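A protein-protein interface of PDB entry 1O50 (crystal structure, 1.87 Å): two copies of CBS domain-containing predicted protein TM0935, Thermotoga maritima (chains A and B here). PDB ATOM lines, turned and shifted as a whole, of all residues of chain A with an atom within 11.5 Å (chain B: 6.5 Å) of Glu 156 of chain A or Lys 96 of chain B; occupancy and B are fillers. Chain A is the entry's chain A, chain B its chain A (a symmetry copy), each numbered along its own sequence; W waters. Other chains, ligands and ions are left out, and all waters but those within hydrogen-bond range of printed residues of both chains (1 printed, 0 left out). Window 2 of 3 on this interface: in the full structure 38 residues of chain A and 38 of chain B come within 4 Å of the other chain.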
ATOM      1  N   HIS A  10     -16.553  25.657  14.706  1.00  0.00           N
ATOM      2  CA  HIS A  10     -16.922  24.522  15.630  1.00  0.00           C
ATOM      3  C   HIS A  10     -18.399  24.599  16.116  1.00  0.00           C
ATOM      4  O   HIS A  10     -18.739  25.407  17.021  1.00  0.00           O
ATOM      5  CB  HIS A  10     -16.031  24.490  16.870  1.00  0.00           C
ATOM      6  CG  HIS A  10     -16.309  23.331  17.779  1.00  0.00           C
ATOM      7  ND1 HIS A  10     -16.168  22.019  17.374  1.00  0.00           N
ATOM      8  CD2 HIS A  10     -16.677  23.281  19.080  1.00  0.00           C
ATOM      9  CE1 HIS A  10     -16.441  21.214  18.388  1.00  0.00           C
ATOM     10  NE2 HIS A  10     -16.775  21.956  19.429  1.00  0.00           N
ATOM     11  N   HIS A  11     -19.233  23.756  15.519  1.00  0.00           N
ATOM     12  CA  HIS A  11     -20.671  23.657  15.792  1.00  0.00           C
ATOM     13  C   HIS A  11     -21.487  24.926  15.565  1.00  0.00           C
ATOM     14  O   HIS A  11     -22.654  24.970  15.950  1.00  0.00           O
ATOM     15  CB  HIS A  11     -20.944  23.099  17.200  1.00  0.00           C
ATOM     16  CG  HIS A  11     -20.408  21.724  17.415  1.00  0.00           C
ATOM     17  ND1 HIS A  11     -20.263  21.177  18.671  1.00  0.00           N
ATOM     18  CD2 HIS A  11     -19.939  20.803  16.543  1.00  0.00           C
ATOM     19  CE1 HIS A  11     -19.765  19.960  18.560  1.00  0.00           C
ATOM     20  NE2 HIS A  11     -19.553  19.709  17.279  1.00  0.00           N
ATOM     21  N   HIS A  12     -20.895  25.925  14.922  1.00  0.00           N
ATOM     22  CA  HIS A  12     -21.595  27.160  14.554  1.00  0.00           C
ATOM     23  C   HIS A  12     -22.387  27.827  15.700  1.00  0.00           C
ATOM     24  O   HIS A  12     -23.485  28.328  15.483  1.00  0.00           O
ATOM     25  CB  HIS A  12     -22.514  26.878  13.370  1.00  0.00           C
ATOM     26  CG  HIS A  12     -21.818  26.233  12.217  1.00  0.00           C
ATOM     27  ND1 HIS A  12     -21.715  24.862  12.088  1.00  0.00           N
ATOM     28  CD2 HIS A  12     -21.148  26.763  11.172  1.00  0.00           C
ATOM     29  CE1 HIS A  12     -21.036  24.581  10.994  1.00  0.00           C
ATOM     30  NE2 HIS A  12     -20.684  25.716  10.418  1.00  0.00           N
ATOM     31  N   MET A  13     -21.842  27.773  16.918  1.00  0.00           N
ATOM     32  CA  MET A  13     -22.437  28.425  18.088  1.00  0.00           C
ATOM     33  C   MET A  13     -22.363  29.955  18.005  1.00  0.00           C
ATOM     34  O   MET A  13     -21.437  30.523  17.437  1.00  0.00           O
ATOM     35  CB  MET A  13     -21.736  27.980  19.381  1.00  0.00           C
ATOM     36  CG  MET A  13     -22.072  26.562  19.821  1.00  0.00           C
ATOM     37  SD  MET A  13     -21.054  25.919  21.167  1.00  0.00           S
ATOM     38  CE  MET A  13     -19.600  25.542  20.378  1.00  0.00           C
ATOM     39  N   ILE A 147     -17.892  30.247  27.846  1.00  0.00           N
ATOM     40  CA  ILE A 147     -17.256  29.728  26.643  1.00  0.00           C
ATOM     41  C   ILE A 147     -16.626  28.390  26.941  1.00  0.00           C
ATOM     42  O   ILE A 147     -16.792  27.453  26.171  1.00  0.00           O
ATOM     43  CB  ILE A 147     -16.255  30.732  26.053  1.00  0.00           C
ATOM     44  CG1 ILE A 147     -16.974  31.998  25.596  1.00  0.00           C
ATOM     45  CG2 ILE A 147     -15.525  30.162  24.828  1.00  0.00           C
ATOM     46  CD1 ILE A 147     -16.098  32.999  24.943  1.00  0.00           C
ATOM     47  N   LEU A 148     -15.935  28.283  28.072  1.00  0.00           N
ATOM     48  CA  LEU A 148     -15.324  27.028  28.468  1.00  0.00           C
ATOM     49  C   LEU A 148     -16.338  25.921  28.690  1.00  0.00           C
ATOM     50  O   LEU A 148     -16.113  24.794  28.266  1.00  0.00           O
ATOM     51  CB  LEU A 148     -14.451  27.187  29.713  1.00  0.00           C
ATOM     52  CG  LEU A 148     -13.179  27.999  29.445  1.00  0.00           C
ATOM     53  CD1 LEU A 148     -12.430  28.322  30.767  1.00  0.00           C
ATOM     54  CD2 LEU A 148     -12.210  27.331  28.435  1.00  0.00           C
ATOM     55  N   LEU A 149     -17.430  26.261  29.357  1.00  0.00           N
ATOM     56  CA  LEU A 149     -18.508  25.349  29.607  1.00  0.00           C
ATOM     57  C   LEU A 149     -19.021  24.774  28.280  1.00  0.00           C
ATOM     58  O   LEU A 149     -19.092  23.565  28.104  1.00  0.00           O
ATOM     59  CB  LEU A 149     -19.617  26.096  30.334  1.00  0.00           C
ATOM     60  CG  LEU A 149     -20.743  25.267  30.992  1.00  0.00           C
ATOM     61  CD1 LEU A 149     -21.568  26.150  31.830  1.00  0.00           C
ATOM     62  CD2 LEU A 149     -21.648  24.472  29.950  1.00  0.00           C
ATOM     63  N   ALA A 150     -19.402  25.662  27.369  1.00  0.00           N
ATOM     64  CA  ALA A 150     -19.889  25.302  26.042  1.00  0.00           C
ATOM     65  C   ALA A 150     -18.972  24.344  25.323  1.00  0.00           C
ATOM     66  O   ALA A 150     -19.400  23.359  24.756  1.00  0.00           O
ATOM     67  CB  ALA A 150     -19.980  26.552  25.207  1.00  0.00           C
ATOM     68  N   LEU A 151     -17.689  24.676  25.320  1.00  0.00           N
ATOM     69  CA  LEU A 151     -16.726  23.920  24.533  1.00  0.00           C
ATOM     70  C   LEU A 151     -16.402  22.559  25.093  1.00  0.00           C
ATOM     71  O   LEU A 151     -16.313  21.599  24.334  1.00  0.00           O
ATOM     72  CB  LEU A 151     -15.460  24.721  24.348  1.00  0.00           C
ATOM     73  CG  LEU A 151     -15.618  25.956  23.448  1.00  0.00           C
ATOM     74  CD1 LEU A 151     -14.279  26.688  23.513  1.00  0.00           C
ATOM     75  CD2 LEU A 151     -16.018  25.612  22.033  1.00  0.00           C
ATOM     76  N   TRP A 152     -16.255  22.464  26.414  1.00  0.00           N
ATOM     77  CA  TRP A 152     -15.837  21.223  27.049  1.00  0.00           C
ATOM     78  C   TRP A 152     -16.939  20.336  27.591  1.00  0.00           C
ATOM     79  O   TRP A 152     -16.700  19.142  27.808  1.00  0.00           O
ATOM     80  CB  TRP A 152     -14.890  21.534  28.187  1.00  0.00           C
ATOM     81  CG  TRP A 152     -13.548  22.013  27.685  1.00  0.00           C
ATOM     82  CD1 TRP A 152     -13.114  23.287  27.694  1.00  0.00           C
ATOM     83  CD2 TRP A 152     -12.498  21.229  27.092  1.00  0.00           C
ATOM     84  NE1 TRP A 152     -11.873  23.361  27.112  1.00  0.00           N
ATOM     85  CE2 TRP A 152     -11.473  22.107  26.749  1.00  0.00           C
ATOM     86  CE3 TRP A 152     -12.324  19.864  26.825  1.00  0.00           C
ATOM     87  CZ2 TRP A 152     -10.262  21.677  26.159  1.00  0.00           C
ATOM     88  CZ3 TRP A 152     -11.135  19.428  26.258  1.00  0.00           C
ATOM     89  CH2 TRP A 152     -10.125  20.341  25.916  1.00  0.00           C
ATOM     90  N   LYS A 153     -18.125  20.897  27.796  1.00  0.00           N
ATOM     91  CA  LYS A 153     -19.290  20.114  28.213  1.00  0.00           C
ATOM     92  C   LYS A 153     -20.112  19.622  27.021  1.00  0.00           C
ATOM     93  O   LYS A 153     -20.947  18.747  27.170  1.00  0.00           O
ATOM     94  CB  LYS A 153     -20.189  20.927  29.111  1.00  0.00           C
ATOM     95  CG  LYS A 153     -19.561  21.448  30.390  1.00  0.00           C
ATOM     96  CD  LYS A 153     -18.875  20.343  31.239  1.00  0.00           C
ATOM     97  CE  LYS A 153     -19.867  19.372  31.849  1.00  0.00           C
ATOM     98  NZ  LYS A 153     -19.167  18.294  32.594  1.00  0.00           N
ATOM     99  N   GLY A 154     -19.907  20.236  25.845  1.00  0.00           N
ATOM    100  CA  GLY A 154     -20.603  19.831  24.641  1.00  0.00           C
ATOM    101  C   GLY A 154     -19.781  18.782  23.917  1.00  0.00           C
ATOM    102  O   GLY A 154     -18.697  18.410  24.377  1.00  0.00           O
ATOM    103  N   ARG A 155     -20.292  18.280  22.799  1.00  0.00           N
ATOM    104  CA  ARG A 155     -19.656  17.174  22.100  1.00  0.00           C
ATOM    105  C   ARG A 155     -18.365  17.656  21.515  1.00  0.00           C
ATOM    106  O   ARG A 155     -18.343  18.695  20.895  1.00  0.00           O
ATOM    107  CB  ARG A 155     -20.536  16.598  20.982  1.00  0.00           C
ATOM    108  CG  ARG A 155     -20.049  15.255  20.521  1.00  0.00           C
ATOM    109  CD  ARG A 155     -20.872  14.576  19.450  1.00  0.00           C
ATOM    110  NE  ARG A 155     -20.617  15.139  18.128  1.00  0.00           N
ATOM    111  CZ  ARG A 155     -21.187  14.699  17.016  1.00  0.00           C
ATOM    112  NH1 ARG A 155     -22.029  13.686  17.066  1.00  0.00           N
ATOM    113  NH2 ARG A 155     -20.922  15.288  15.862  1.00  0.00           N
ATOM    114  N   GLU A 156     -17.284  16.906  21.702  1.00  0.00           N
ATOM    115  CA  GLU A 156     -15.994  17.332  21.158  1.00  0.00           C
ATOM    116  C   GLU A 156     -15.929  17.377  19.625  1.00  0.00           C
ATOM    117  O   GLU A 156     -15.391  18.324  19.064  1.00  0.00           O
ATOM    118  CB  GLU A 156     -14.844  16.486  21.670  1.00  0.00           C
ATOM    119  CG  GLU A 156     -13.514  16.995  21.089  1.00  0.00           C
ATOM    120  CD  GLU A 156     -12.285  16.391  21.741  1.00  0.00           C
ATOM    121  OE1 GLU A 156     -12.437  15.437  22.529  1.00  0.00           O
ATOM    122  OE2 GLU A 156     -11.165  16.840  21.424  1.00  0.00           O
ATOM    123  N   LYS A 157     -16.433  16.335  18.966  1.00  0.00           N
ATOM    124  CA  LYS A 157     -16.434  16.256  17.502  1.00  0.00           C
ATOM    125  C   LYS A 157     -17.609  17.073  16.960  1.00  0.00           C
ATOM    126  O   LYS A 157     -17.570  17.663  15.884  1.00  0.00           O
ATOM    127  CB  LYS A 157     -16.537  14.789  17.047  1.00  0.00           C
ATOM    128  CG  LYS A 157     -16.514  14.571  15.513  1.00  0.00           C
ATOM    129  CD  LYS A 157     -16.552  13.072  15.153  1.00  0.00           C
ATOM    130  CE  LYS A 157     -16.662  12.842  13.621  1.00  0.00           C
ATOM    131  OXT LYS A 157     -18.661  17.172  17.582  1.00  0.00           O
ATOM    132  N   ASP B  32      -3.106  13.955  35.830  1.00  0.00           N
ATOM    133  CA  ASP B  32      -3.945  13.191  34.894  1.00  0.00           C
ATOM    134  C   ASP B  32      -5.407  13.598  34.935  1.00  0.00           C
ATOM    135  O   ASP B  32      -6.257  12.914  34.385  1.00  0.00           O
ATOM    136  CB  ASP B  32      -3.843  11.680  35.130  1.00  0.00           C
ATOM    137  CG  ASP B  32      -4.392  11.246  36.482  1.00  0.00           C
ATOM    138  OD1 ASP B  32      -4.728  12.091  37.313  1.00  0.00           O
ATOM    139  OD2 ASP B  32      -4.526  10.059  36.816  1.00  0.00           O
ATOM    140  N   THR B  33      -5.701  14.702  35.609  1.00  0.00           N
ATOM    141  CA  THR B  33      -7.050  15.225  35.691  1.00  0.00           C
ATOM    142  C   THR B  33      -7.489  15.725  34.303  1.00  0.00           C
ATOM    143  O   THR B  33      -6.796  16.545  33.708  1.00  0.00           O
ATOM    144  CB  THR B  33      -7.106  16.363  36.731  1.00  0.00           C
ATOM    145  OG1 THR B  33      -6.829  15.854  38.068  1.00  0.00           O
ATOM    146  CG2 THR B  33      -8.526  16.898  36.789  1.00  0.00           C
ATOM    147  N   PRO B  34      -8.601  15.199  33.773  1.00  0.00           N
ATOM    148  CA  PRO B  34      -9.095  15.634  32.477  1.00  0.00           C
ATOM    149  C   PRO B  34      -9.506  17.101  32.452  1.00  0.00           C
ATOM    150  O   PRO B  34      -9.999  17.631  33.410  1.00  0.00           O
ATOM    151  CB  PRO B  34     -10.308  14.728  32.247  1.00  0.00           C
ATOM    152  CG  PRO B  34     -10.037  13.541  33.085  1.00  0.00           C
ATOM    153  CD  PRO B  34      -9.418  14.099  34.328  1.00  0.00           C
ATOM    154  N   ILE B  35      -9.324  17.743  31.305  1.00  0.00           N
ATOM    155  CA  ILE B  35      -9.569  19.163  31.195  1.00  0.00           C
ATOM    156  C   ILE B  35     -11.021  19.429  31.447  1.00  0.00           C
ATOM    157  O   ILE B  35     -11.370  20.418  32.109  1.00  0.00           O
ATOM    158  CB  ILE B  35      -9.117  19.661  29.829  1.00  0.00           C
ATOM    159  CG1 ILE B  35      -7.587  19.622  29.790  1.00  0.00           C
ATOM    160  CG2 ILE B  35      -9.641  21.068  29.556  1.00  0.00           C
ATOM    161  CD1 ILE B  35      -6.957  19.945  28.408  1.00  0.00           C
ATOM    162  N   GLU B  36     -11.890  18.534  30.988  1.00  0.00           N
ATOM    163  CA  GLU B  36     -13.323  18.705  31.288  1.00  0.00           C
ATOM    164  C   GLU B  36     -13.567  18.761  32.832  1.00  0.00           C
ATOM    165  O   GLU B  36     -14.363  19.561  33.317  1.00  0.00           O
ATOM    166  CB  GLU B  36     -14.149  17.624  30.623  1.00  0.00           C
ATOM    167  CG  GLU B  36     -15.640  17.891  30.818  1.00  0.00           C
ATOM    168  CD  GLU B  36     -16.619  16.893  30.193  1.00  0.00           C
ATOM    169  OE1 GLU B  36     -16.238  16.091  29.351  1.00  0.00           O
ATOM    170  OE2 GLU B  36     -17.835  16.927  30.547  1.00  0.00           O
ATOM    171  N   HIS B  75      -7.503  24.483  20.160  1.00  0.00           N
ATOM    172  CA  HIS B  75      -7.991  23.132  19.988  1.00  0.00           C
ATOM    173  C   HIS B  75      -9.295  23.083  19.185  1.00  0.00           C
ATOM    174  O   HIS B  75      -9.446  22.232  18.327  1.00  0.00           O
ATOM    175  CB  HIS B  75      -8.256  22.494  21.365  1.00  0.00           C
ATOM    176  CG  HIS B  75      -8.689  21.067  21.281  1.00  0.00           C
ATOM    177  ND1 HIS B  75      -7.823  20.053  20.939  1.00  0.00           N
ATOM    178  CD2 HIS B  75      -9.894  20.482  21.495  1.00  0.00           C
ATOM    179  CE1 HIS B  75      -8.474  18.902  20.957  1.00  0.00           C
ATOM    180  NE2 HIS B  75      -9.730  19.136  21.275  1.00  0.00           N
ATOM    181  N   PHE B  76     -10.236  23.980  19.495  1.00  0.00           N
ATOM    182  CA  PHE B  76     -11.565  23.948  18.892  1.00  0.00           C
ATOM    183  C   PHE B  76     -11.710  24.802  17.637  1.00  0.00           C
ATOM    184  O   PHE B  76     -12.491  24.460  16.763  1.00  0.00           O
ATOM    185  CB  PHE B  76     -12.610  24.333  19.926  1.00  0.00           C
ATOM    186  CG  PHE B  76     -12.837  23.279  20.952  1.00  0.00           C
ATOM    187  CD1 PHE B  76     -13.577  22.148  20.642  1.00  0.00           C
ATOM    188  CD2 PHE B  76     -12.327  23.394  22.225  1.00  0.00           C
ATOM    189  CE1 PHE B  76     -13.772  21.168  21.578  1.00  0.00           C
ATOM    190  CE2 PHE B  76     -12.546  22.436  23.152  1.00  0.00           C
ATOM    191  CZ  PHE B  76     -13.254  21.304  22.816  1.00  0.00           C
ATOM    192  N   LEU B  93      -3.620  18.650  21.615  1.00  0.00           N
ATOM    193  CA  LEU B  93      -4.007  17.917  22.800  1.00  0.00           C
ATOM    194  C   LEU B  93      -4.255  16.450  22.427  1.00  0.00           C
ATOM    195  O   LEU B  93      -4.884  16.164  21.412  1.00  0.00           O
ATOM    196  CB  LEU B  93      -5.245  18.533  23.425  1.00  0.00           C
ATOM    197  CG  LEU B  93      -5.082  19.971  23.913  1.00  0.00           C
ATOM    198  CD1 LEU B  93      -6.420  20.458  24.396  1.00  0.00           C
ATOM    199  CD2 LEU B  93      -4.033  20.051  25.020  1.00  0.00           C
ATOM    200  N   ILE B  94      -3.740  15.541  23.257  1.00  0.00           N
ATOM    201  CA  ILE B  94      -3.905  14.096  23.070  1.00  0.00           C
ATOM    202  C   ILE B  94      -4.676  13.461  24.261  1.00  0.00           C
ATOM    203  O   ILE B  94      -5.793  12.959  24.095  1.00  0.00           O
ATOM    204  CB  ILE B  94      -2.494  13.443  22.871  1.00  0.00           C
ATOM    205  CG1 ILE B  94      -1.712  14.154  21.749  1.00  0.00           C
ATOM    206  CG2 ILE B  94      -2.593  11.959  22.589  1.00  0.00           C
ATOM    207  CD1 ILE B  94      -2.146  13.809  20.347  1.00  0.00           C
ATOM    208  N   ALA B  95      -4.085  13.491  25.450  1.00  0.00           N
ATOM    209  CA  ALA B  95      -4.744  13.016  26.688  1.00  0.00           C
ATOM    210  C   ALA B  95      -5.856  13.971  27.155  1.00  0.00           C
ATOM    211  O   ALA B  95      -6.851  13.550  27.795  1.00  0.00           O
ATOM    212  CB  ALA B  95      -3.683  12.813  27.789  1.00  0.00           C
ATOM    213  N   LYS B  96      -5.744  15.245  26.752  1.00  0.00           N
ATOM    214  CA  LYS B  96      -6.580  16.326  27.246  1.00  0.00           C
ATOM    215  C   LYS B  96      -6.629  16.325  28.787  1.00  0.00           C
ATOM    216  O   LYS B  96      -7.662  16.133  29.406  1.00  0.00           O
ATOM    217  CB  LYS B  96      -7.964  16.242  26.592  1.00  0.00           C
ATOM    218  CG  LYS B  96      -7.893  16.371  25.040  1.00  0.00           C
ATOM    219  CD  LYS B  96      -8.897  15.451  24.340  1.00  0.00           C
ATOM    220  CE  LYS B  96      -8.616  15.436  22.852  1.00  0.00           C
ATOM    221  NZ  LYS B  96      -9.616  14.624  22.074  1.00  0.00           N
ATOM    222  N   ASN B  97      -5.482  16.507  29.405  1.00  0.00           N
ATOM    223  CA  ASN B  97      -5.425  16.564  30.857  1.00  0.00           C
ATOM    224  C   ASN B  97      -4.577  17.755  31.358  1.00  0.00           C
ATOM    225  O   ASN B  97      -3.977  18.487  30.562  1.00  0.00           O
ATOM    226  CB  ASN B  97      -5.010  15.212  31.458  1.00  0.00           C
ATOM    227  CG  ASN B  97      -3.570  14.772  31.082  1.00  0.00           C
ATOM    228  OD1 ASN B  97      -2.672  15.576  30.879  1.00  0.00           O
ATOM    229  ND2 ASN B  97      -3.364  13.479  31.067  1.00  0.00           N
ATOM    230  N   ALA B  98      -4.567  17.950  32.670  1.00  0.00           N
ATOM    231  CA  ALA B  98      -3.782  19.003  33.281  1.00  0.00           C
ATOM    232  C   ALA B  98      -2.310  18.993  32.888  1.00  0.00           C
ATOM    233  O   ALA B  98      -1.742  20.052  32.610  1.00  0.00           O
ATOM    234  CB  ALA B  98      -3.887  18.880  34.799  1.00  0.00           C
ATOM    235  N   GLU B 100      -0.689  18.261  30.234  1.00  0.00           N
ATOM    236  CA  GLU B 100      -0.427  18.711  28.870  1.00  0.00           C
ATOM    237  C   GLU B 100      -0.475  20.212  28.737  1.00  0.00           C
ATOM    238  O   GLU B 100       0.138  20.773  27.796  1.00  0.00           O
ATOM    239  CB  GLU B 100      -1.486  18.147  27.912  1.00  0.00           C
ATOM    240  CG  GLU B 100      -1.359  16.674  27.611  1.00  0.00           C
ATOM    241  CD  GLU B 100      -2.328  16.156  26.540  1.00  0.00           C
ATOM    242  OE1 GLU B 100      -3.512  16.613  26.450  1.00  0.00           O
ATOM    243  OE2 GLU B 100      -1.905  15.206  25.839  1.00  0.00           O
HETATM  244  O   HOH W   1     -13.046  21.774  16.291  1.00  0.00           O
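Of chain A, only Glu 156 (2.8 Å) comes within 4 Å of Lys 96 of chain B.
Ile 35 of chain B touches just one residue of chain A: Trp 152.
No residue of chain A comes within 4 Å of Ala 95 of chain B.
No residue of chain A comes within 4 Å of Asn 97 of chain B.
No residue of chain A comes within 4 Å of Ala 98 of chain B.
Printed residues of chain B within 4 Å of Leu 151 of chain A: Phe 76 (3.4 Å).
Of the printed residues of chain B, Lys 153 of chain A touches Glu 36.
Of the printed residues of chain A, Glu 36 of chain B touches Trp 152 (3.3 Å) and Lys 153 (2.8 Å).
Thr 33 of chain B touches none of the printed residues of chain A.
The nearest residue of chain A that does not touch Lys 96 of chain B is Trp 152 of chain A (4.5 Å).
The nearest printed residue of chain B that does not touch Lys 153 of chain A is Phe 76 of chain B (7.0 Å).
Water W1 bridges O of Phe 76 of chain B (2.8 Å) and ND1 of His 10 of chain A (3.3 Å).
Among the printed residues, pairs that only touch across the chains: His 10 of chain A with Phe 76 of chain B (3.4 Å), Leu 151 of chain A with Phe 76 of chain B (3.4 Å), Trp 152 of chain A with Ile 35 of chain B (3.5 Å) and Trp 152 of chain A with Phe 76 of chain B (3.8 Å).
The backbone NH (N) of Ile 35 of chain B lies within hydrogen-bond range of the backbone carbonyl oxygen (O) of Lys 96 of chain B.
The backbone NH (N) of Lys 96 of chain B sits at hydrogen-bond distance from the side-chain carboxylate (OE1) of Glu 100 of chain B (2.6 Å).
Of the 14 printed residues of chain B, 5 touch a printed residue of chain A.
Hydrophobic or aromatic side chains of chain B that line the printed part of chain A: Ile 35, His 75 and Phe 76.
Of the 15 printed residues of chain A, 5 touch a printed residue of chain B.
Hydrophobic or aromatic side chains of chain A that line the printed part of chain B: His 10, Leu 151 and Trp 152.
Among the printed residues, Asp or Glu carboxylates within 4 Å of a Lys or Arg side-chain nitrogen of the other chain: Lys 153 of chain A with Glu 36 of chain B (2.8 Å) and Glu 156 of chain A with Lys 96 of chain B (2.8 Å).
No position is printed for both chains.
NZ of Lys 153 of chain A is in salt-bridge range of OE2 of Glu 36 of chain B, at 2.8 Å.
NE2 of His 75 of chain B sits at hydrogen-bond distance from OE2 of Glu 156 of chain A (2.7 Å).
The side-chain amino group of Lys 96 of chain B is in salt-bridge range of the side-chain carboxylate of Glu 156 of chain A (2.8 Å).
O of Trp 152 of chain A lies close to OE1 of Glu 36 of chain B.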
